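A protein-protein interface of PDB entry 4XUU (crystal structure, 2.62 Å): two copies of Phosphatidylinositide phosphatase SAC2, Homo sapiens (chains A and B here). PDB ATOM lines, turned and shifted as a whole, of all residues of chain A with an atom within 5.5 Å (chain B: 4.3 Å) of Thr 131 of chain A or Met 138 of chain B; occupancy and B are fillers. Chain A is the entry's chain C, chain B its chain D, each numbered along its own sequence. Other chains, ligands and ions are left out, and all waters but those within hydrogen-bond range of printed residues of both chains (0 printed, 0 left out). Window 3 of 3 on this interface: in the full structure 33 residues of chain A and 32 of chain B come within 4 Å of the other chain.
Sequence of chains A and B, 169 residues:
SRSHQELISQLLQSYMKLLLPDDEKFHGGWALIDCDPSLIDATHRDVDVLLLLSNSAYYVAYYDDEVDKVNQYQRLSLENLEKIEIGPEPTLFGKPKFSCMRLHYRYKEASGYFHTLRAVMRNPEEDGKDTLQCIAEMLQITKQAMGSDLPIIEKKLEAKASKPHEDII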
ATOM      1  N   TRP A  30     -22.687 -21.115  10.047  1.00  0.00           N
ATOM      2  CA  TRP A  30     -21.508 -21.355   9.205  1.00  0.00           C
ATOM      3  C   TRP A  30     -21.633 -20.655   7.868  1.00  0.00           C
ATOM      4  O   TRP A  30     -22.729 -20.519   7.331  1.00  0.00           O
ATOM      5  CB  TRP A  30     -21.304 -22.862   8.965  1.00  0.00           C
ATOM      6  CG  TRP A  30     -21.264 -23.669  10.218  1.00  0.00           C
ATOM      7  CD1 TRP A  30     -20.155 -24.021  10.929  1.00  0.00           C
ATOM      8  CD2 TRP A  30     -22.386 -24.218  10.921  1.00  0.00           C
ATOM      9  NE1 TRP A  30     -20.515 -24.761  12.033  1.00  0.00           N
ATOM     10  CE2 TRP A  30     -21.878 -24.896  12.053  1.00  0.00           C
ATOM     11  CE3 TRP A  30     -23.770 -24.207  10.704  1.00  0.00           C
ATOM     12  CZ2 TRP A  30     -22.706 -25.552  12.969  1.00  0.00           C
ATOM     13  CZ3 TRP A  30     -24.596 -24.856  11.616  1.00  0.00           C
ATOM     14  CH2 TRP A  30     -24.059 -25.521  12.737  1.00  0.00           C
ATOM     15  N   ALA A 119     -17.643 -26.244   2.169  1.00  0.00           N
ATOM     16  CA  ALA A 119     -16.992 -25.300   3.072  1.00  0.00           C
ATOM     17  C   ALA A 119     -16.133 -24.287   2.325  1.00  0.00           C
ATOM     18  O   ALA A 119     -15.676 -24.549   1.212  1.00  0.00           O
ATOM     19  CB  ALA A 119     -16.161 -26.047   4.105  1.00  0.00           C
ATOM     20  N   MET A 121     -12.911 -23.059   1.704  1.00  0.00           N
ATOM     21  CA  MET A 121     -11.608 -23.664   1.947  1.00  0.00           C
ATOM     22  C   MET A 121     -10.454 -22.943   1.272  1.00  0.00           C
ATOM     23  O   MET A 121     -10.409 -22.809   0.047  1.00  0.00           O
ATOM     24  CB  MET A 121     -11.615 -25.152   1.598  1.00  0.00           C
ATOM     25  CG  MET A 121     -11.031 -26.037   2.692  1.00  0.00           C
ATOM     26  SD  MET A 121     -11.951 -25.802   4.407  1.00  0.00           S
ATOM     27  CE  MET A 121     -10.829 -24.394   5.183  1.00  0.00           C
ATOM     28  N   GLY A 128     -12.077 -30.827   2.934  1.00  0.00           N
ATOM     29  CA  GLY A 128     -13.133 -30.099   3.636  1.00  0.00           C
ATOM     30  C   GLY A 128     -14.239 -30.990   4.174  1.00  0.00           C
ATOM     31  O   GLY A 128     -15.282 -30.497   4.599  1.00  0.00           O
ATOM     32  N   LYS A 129     -14.006 -32.302   4.163  1.00  0.00           N
ATOM     33  CA  LYS A 129     -14.998 -33.284   4.605  1.00  0.00           C
ATOM     34  C   LYS A 129     -15.247 -33.231   6.119  1.00  0.00           C
ATOM     35  O   LYS A 129     -16.398 -33.320   6.564  1.00  0.00           O
ATOM     36  CB  LYS A 129     -14.585 -34.695   4.170  1.00  0.00           C
ATOM     37  CG  LYS A 129     -15.675 -35.751   4.317  1.00  0.00           C
ATOM     38  CD  LYS A 129     -15.336 -37.035   3.567  1.00  0.00           C
ATOM     39  CE  LYS A 129     -14.360 -37.925   4.334  1.00  0.00           C
ATOM     40  NZ  LYS A 129     -13.959 -39.129   3.544  1.00  0.00           N
ATOM     41  N   ASP A 130     -14.169 -33.088   6.891  1.00  0.00           N
ATOM     42  CA  ASP A 130     -14.241 -32.965   8.348  1.00  0.00           C
ATOM     43  C   ASP A 130     -15.173 -31.834   8.784  1.00  0.00           C
ATOM     44  O   ASP A 130     -15.993 -32.016   9.688  1.00  0.00           O
ATOM     45  CB  ASP A 130     -12.846 -32.734   8.944  1.00  0.00           C
ATOM     46  CG  ASP A 130     -11.951 -33.963   8.868  1.00  0.00           C
ATOM     47  OD1 ASP A 130     -12.450 -35.075   8.597  1.00  0.00           O
ATOM     48  OD2 ASP A 130     -10.731 -33.812   9.087  1.00  0.00           O
ATOM     49  N   THR A 131     -15.042 -30.676   8.135  1.00  0.00           N
ATOM     50  CA  THR A 131     -15.885 -29.512   8.404  1.00  0.00           C
ATOM     51  C   THR A 131     -17.365 -29.839   8.205  1.00  0.00           C
ATOM     52  O   THR A 131     -18.198 -29.500   9.047  1.00  0.00           O
ATOM     53  CB  THR A 131     -15.487 -28.315   7.508  1.00  0.00           C
ATOM     54  OG1 THR A 131     -14.103 -28.005   7.709  1.00  0.00           O
ATOM     55  CG2 THR A 131     -16.323 -27.083   7.823  1.00  0.00           C
ATOM     56  N   LEU A 132     -17.677 -30.510   7.099  1.00  0.00           N
ATOM     57  CA  LEU A 132     -19.055 -30.884   6.779  1.00  0.00           C
ATOM     58  C   LEU A 132     -19.584 -31.981   7.703  1.00  0.00           C
ATOM     59  O   LEU A 132     -20.734 -31.937   8.125  1.00  0.00           O
ATOM     60  CB  LEU A 132     -19.183 -31.302   5.309  1.00  0.00           C
ATOM     61  CG  LEU A 132     -18.776 -30.294   4.224  1.00  0.00           C
ATOM     62  CD1 LEU A 132     -18.889 -30.926   2.847  1.00  0.00           C
ATOM     63  CD2 LEU A 132     -19.594 -29.003   4.294  1.00  0.00           C
ATOM     64  N   GLN A 133     -18.741 -32.958   8.023  1.00  0.00           N
ATOM     65  CA  GLN A 133     -19.116 -34.005   8.970  1.00  0.00           C
ATOM     66  C   GLN A 133     -19.549 -33.357  10.288  1.00  0.00           C
ATOM     67  O   GLN A 133     -20.554 -33.748  10.876  1.00  0.00           O
ATOM     68  CB  GLN A 133     -17.955 -34.989   9.171  1.00  0.00           C
ATOM     69  CG  GLN A 133     -18.222 -36.144  10.143  1.00  0.00           C
ATOM     70  CD  GLN A 133     -19.452 -36.979   9.784  1.00  0.00           C
ATOM     71  OE1 GLN A 133     -19.600 -37.445   8.647  1.00  0.00           O
ATOM     72  NE2 GLN A 133     -20.336 -37.178  10.764  1.00  0.00           N
ATOM     73  N   CYS A 134     -18.803 -32.338  10.710  1.00  0.00           N
ATOM     74  CA  CYS A 134     -19.075 -31.600  11.942  1.00  0.00           C
ATOM     75  C   CYS A 134     -20.411 -30.856  11.934  1.00  0.00           C
ATOM     76  O   CYS A 134     -21.172 -30.929  12.911  1.00  0.00           O
ATOM     77  CB  CYS A 134     -17.931 -30.634  12.239  1.00  0.00           C
ATOM     78  SG  CYS A 134     -16.419 -31.492  12.708  1.00  0.00           S
ATOM     79  N   ILE A 135     -20.689 -30.146  10.840  1.00  0.00           N
ATOM     80  CA  ILE A 135     -21.965 -29.449  10.683  1.00  0.00           C
ATOM     81  C   ILE A 135     -23.130 -30.438  10.787  1.00  0.00           C
ATOM     82  O   ILE A 135     -24.049 -30.226  11.575  1.00  0.00           O
ATOM     83  CB  ILE A 135     -22.020 -28.603   9.378  1.00  0.00           C
ATOM     84  CG1 ILE A 135     -21.094 -27.388   9.499  1.00  0.00           C
ATOM     85  CG2 ILE A 135     -23.440 -28.132   9.087  1.00  0.00           C
ATOM     86  CD1 ILE A 135     -20.671 -26.779   8.160  1.00  0.00           C
ATOM     87  N   ALA A 136     -23.060 -31.528  10.021  1.00  0.00           N
ATOM     88  CA  ALA A 136     -24.081 -32.585  10.044  1.00  0.00           C
ATOM     89  C   ALA A 136     -24.269 -33.188  11.434  1.00  0.00           C
ATOM     90  O   ALA A 136     -25.382 -33.554  11.813  1.00  0.00           O
ATOM     91  CB  ALA A 136     -23.746 -33.679   9.040  1.00  0.00           C
ATOM     92  N   TRP B  30     -20.907 -20.194  17.251  1.00  0.00           N
ATOM     93  CA  TRP B  30     -21.429 -21.253  18.120  1.00  0.00           C
ATOM     94  C   TRP B  30     -21.900 -20.699  19.449  1.00  0.00           C
ATOM     95  O   TRP B  30     -21.275 -19.796  20.017  1.00  0.00           O
ATOM     96  CB  TRP B  30     -20.369 -22.337  18.378  1.00  0.00           C
ATOM     97  CG  TRP B  30     -19.758 -22.854  17.129  1.00  0.00           C
ATOM     98  CD1 TRP B  30     -20.187 -23.913  16.379  1.00  0.00           C
ATOM     99  CD2 TRP B  30     -18.620 -22.311  16.452  1.00  0.00           C
ATOM    100  NE1 TRP B  30     -19.376 -24.066  15.276  1.00  0.00           N
ATOM    101  CE2 TRP B  30     -18.408 -23.095  15.298  1.00  0.00           C
ATOM    102  CE3 TRP B  30     -17.756 -21.240  16.712  1.00  0.00           C
ATOM    103  CZ2 TRP B  30     -17.368 -22.845  14.408  1.00  0.00           C
ATOM    104  CZ3 TRP B  30     -16.719 -20.990  15.824  1.00  0.00           C
ATOM    105  CH2 TRP B  30     -16.535 -21.790  14.687  1.00  0.00           C
ATOM    106  N   LEU B  53     -16.386 -16.503  14.763  1.00  0.00           N
ATOM    107  CA  LEU B  53     -15.109 -16.549  14.064  1.00  0.00           C
ATOM    108  C   LEU B  53     -15.178 -15.828  12.713  1.00  0.00           C
ATOM    109  O   LEU B  53     -16.081 -16.081  11.914  1.00  0.00           O
ATOM    110  CB  LEU B  53     -14.641 -18.005  13.889  1.00  0.00           C
ATOM    111  CG  LEU B  53     -13.347 -18.277  13.104  1.00  0.00           C
ATOM    112  CD1 LEU B  53     -12.133 -17.656  13.788  1.00  0.00           C
ATOM    113  CD2 LEU B  53     -13.129 -19.773  12.897  1.00  0.00           C
ATOM    114  N   CYS B 134     -14.366 -30.002  16.712  1.00  0.00           N
ATOM    115  CA  CYS B 134     -14.755 -29.396  15.438  1.00  0.00           C
ATOM    116  C   CYS B 134     -14.547 -27.886  15.436  1.00  0.00           C
ATOM    117  O   CYS B 134     -14.056 -27.324  14.457  1.00  0.00           O
ATOM    118  CB  CYS B 134     -16.212 -29.721  15.115  1.00  0.00           C
ATOM    119  SG  CYS B 134     -16.497 -31.456  14.728  1.00  0.00           S
ATOM    120  N   ILE B 135     -14.923 -27.242  16.538  1.00  0.00           N
ATOM    121  CA  ILE B 135     -14.686 -25.813  16.728  1.00  0.00           C
ATOM    122  C   ILE B 135     -13.184 -25.529  16.722  1.00  0.00           C
ATOM    123  O   ILE B 135     -12.727 -24.614  16.037  1.00  0.00           O
ATOM    124  CB  ILE B 135     -15.323 -25.297  18.045  1.00  0.00           C
ATOM    125  CG1 ILE B 135     -16.832 -25.562  18.057  1.00  0.00           C
ATOM    126  CG2 ILE B 135     -15.033 -23.815  18.242  1.00  0.00           C
ATOM    127  CD1 ILE B 135     -17.473 -25.453  19.436  1.00  0.00           C
ATOM    128  N   ALA B 136     -12.426 -26.328  17.475  1.00  0.00           N
ATOM    129  CA  ALA B 136     -10.969 -26.203  17.545  1.00  0.00           C
ATOM    130  C   ALA B 136     -10.349 -26.303  16.166  1.00  0.00           C
ATOM    131  O   ALA B 136      -9.438 -25.545  15.829  1.00  0.00           O
ATOM    132  CB  ALA B 136     -10.392 -27.264  18.448  1.00  0.00           C
ATOM    133  N   GLU B 137     -10.863 -27.233  15.369  1.00  0.00           N
ATOM    134  CA  GLU B 137     -10.334 -27.474  14.041  1.00  0.00           C
ATOM    135  C   GLU B 137     -10.668 -26.350  13.069  1.00  0.00           C
ATOM    136  O   GLU B 137      -9.944 -26.140  12.102  1.00  0.00           O
ATOM    137  CB  GLU B 137     -10.778 -28.838  13.511  1.00  0.00           C
ATOM    138  CG  GLU B 137      -9.949 -29.988  14.084  1.00  0.00           C
ATOM    139  CD  GLU B 137     -10.415 -31.359  13.621  1.00  0.00           C
ATOM    140  OE1 GLU B 137     -10.160 -32.347  14.347  1.00  0.00           O
ATOM    141  OE2 GLU B 137     -11.030 -31.453  12.536  1.00  0.00           O
ATOM    142  N   MET B 138     -11.742 -25.612  13.328  1.00  0.00           N
ATOM    143  CA  MET B 138     -12.027 -24.454  12.486  1.00  0.00           C
ATOM    144  C   MET B 138     -11.194 -23.238  12.882  1.00  0.00           C
ATOM    145  O   MET B 138     -10.737 -22.492  12.020  1.00  0.00           O
ATOM    146  CB  MET B 138     -13.513 -24.116  12.416  1.00  0.00           C
ATOM    147  CG  MET B 138     -13.839 -23.319  11.152  1.00  0.00           C
ATOM    148  SD  MET B 138     -15.706 -22.839  10.975  1.00  0.00           S
ATOM    149  CE  MET B 138     -16.414 -24.632  10.648  1.00  0.00           C
ATOM    150  N   LEU B 139     -10.988 -23.058  14.183  1.00  0.00           N
ATOM    151  CA  LEU B 139     -10.099 -22.017  14.690  1.00  0.00           C
ATOM    152  C   LEU B 139      -8.655 -22.240  14.237  1.00  0.00           C
ATOM    153  O   LEU B 139      -7.950 -21.281  13.906  1.00  0.00           O
ATOM    154  CB  LEU B 139     -10.167 -21.940  16.220  1.00  0.00           C
ATOM    155  CG  LEU B 139     -11.491 -21.495  16.848  1.00  0.00           C
ATOM    156  CD1 LEU B 139     -11.578 -21.937  18.291  1.00  0.00           C
ATOM    157  CD2 LEU B 139     -11.672 -19.991  16.737  1.00  0.00           C
ATOM    158  N   GLN B 140      -8.230 -23.507  14.220  1.00  0.00           N
ATOM    159  CA  GLN B 140      -6.881 -23.887  13.796  1.00  0.00           C
ATOM    160  C   GLN B 140      -6.672 -23.607  12.309  1.00  0.00           C
ATOM    161  O   GLN B 140      -5.710 -22.942  11.922  1.00  0.00           O
ATOM    162  CB  GLN B 140      -6.611 -25.367  14.110  1.00  0.00           C
ATOM    163  CG  GLN B 140      -5.171 -25.827  13.861  1.00  0.00           C
ATOM    164  CD  GLN B 140      -4.974 -27.323  14.075  1.00  0.00           C
ATOM    165  OE1 GLN B 140      -5.656 -28.146  13.468  1.00  0.00           O
ATOM    166  NE2 GLN B 140      -4.027 -27.679  14.934  1.00  0.00           N
ATOM    167  N   ILE B 141      -7.595 -24.104  11.490  1.00  0.00           N
ATOM    168  CA  ILE B 141      -7.502 -23.999  10.035  1.00  0.00           C
ATOM    169  C   ILE B 141      -7.593 -22.542   9.551  1.00  0.00           C
ATOM    170  O   ILE B 141      -7.027 -22.194   8.514  1.00  0.00           O
ATOM    171  CB  ILE B 141      -8.572 -24.901   9.348  1.00  0.00           C
ATOM    172  CG1 ILE B 141      -8.136 -25.315   7.946  1.00  0.00           C
ATOM    173  CG2 ILE B 141      -9.950 -24.237   9.325  1.00  0.00           C
ATOM    174  CD1 ILE B 141      -8.867 -26.548   7.444  1.00  0.00           C
ATOM    175  N   THR B 142      -8.292 -21.705  10.317  1.00  0.00           N
ATOM    176  CA  THR B 142      -8.457 -20.289   9.999  1.00  0.00           C
ATOM    177  C   THR B 142      -7.210 -19.488  10.380  1.00  0.00           C
ATOM    178  O   THR B 142      -6.757 -18.637   9.607  1.00  0.00           O
ATOM    179  CB  THR B 142      -9.724 -19.700  10.673  1.00  0.00           C
ATOM    180  OG1 THR B 142     -10.855 -20.521  10.357  1.00  0.00           O
ATOM    181  CG2 THR B 142     -10.008 -18.286  10.187  1.00  0.00           C
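Trp 30 of chain B touches its own counterpart, Trp 30 of chain A. Cys 134 of chain A touches its own counterpart, Cys 134 of chain B. 4 positions are printed for both chains.
O of Met 138 of chain B is in hydrogen-bond range of OG1 of Thr 142 of chain B (2.6 Å).
The side-chain sulfur (SG) of Cys 134 of chain B is disulfide-bonded to the side-chain sulfur (SG) of Cys 134 of chain A (2.0 Å).
Of the 12 printed residues of chain A, 4 touch a printed residue of chain B. Hydrophobic or aromatic side chains of chain A within 4 Å of the printed part of chain B: Trp 30 and Met 121. Hydrophobic or aromatic side chains of chain B that line the printed part of chain A: Trp 30, Met 138 and Ile 141. Among the printed residues, 5 pairs touch across the chains. Among the printed residues, no Asp or Glu carboxylate lies within 4 Å of a Lys or Arg side-chain nitrogen of the other chain.
Trp 30 of chain A touches Trp 30 of chain B. Met 138 of chain B touches Trp 30 of chain A (CE to CD1, 3.8 Å). CE of Met 121 of chain A touches CD1 of Ile 141 of chain B, at 3.7 Å. CG2 of Thr 131 of chain A touches CE of Met 138 of chain B (3.7 Å).
Thr 131 of chain A touches just one residue of chain B: Met 138. Met 138 of chain B touches just these residues of chain A: Trp 30 and Thr 131. Of the printed residues of chain B, Cys 134 of chain A touches Cys 134 (2.0 Å). Of the printed residues of chain B, Trp 30 of chain A touches Trp 30 and Met 138. Printed residues of chain A within 4 Å of Cys 134 of chain B: Cys 134. Of the printed residues of chain B, Met 121 of chain A touches Ile 141 (3.7 Å). Leu 139 of chain B touches none of the printed residues of chain A.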
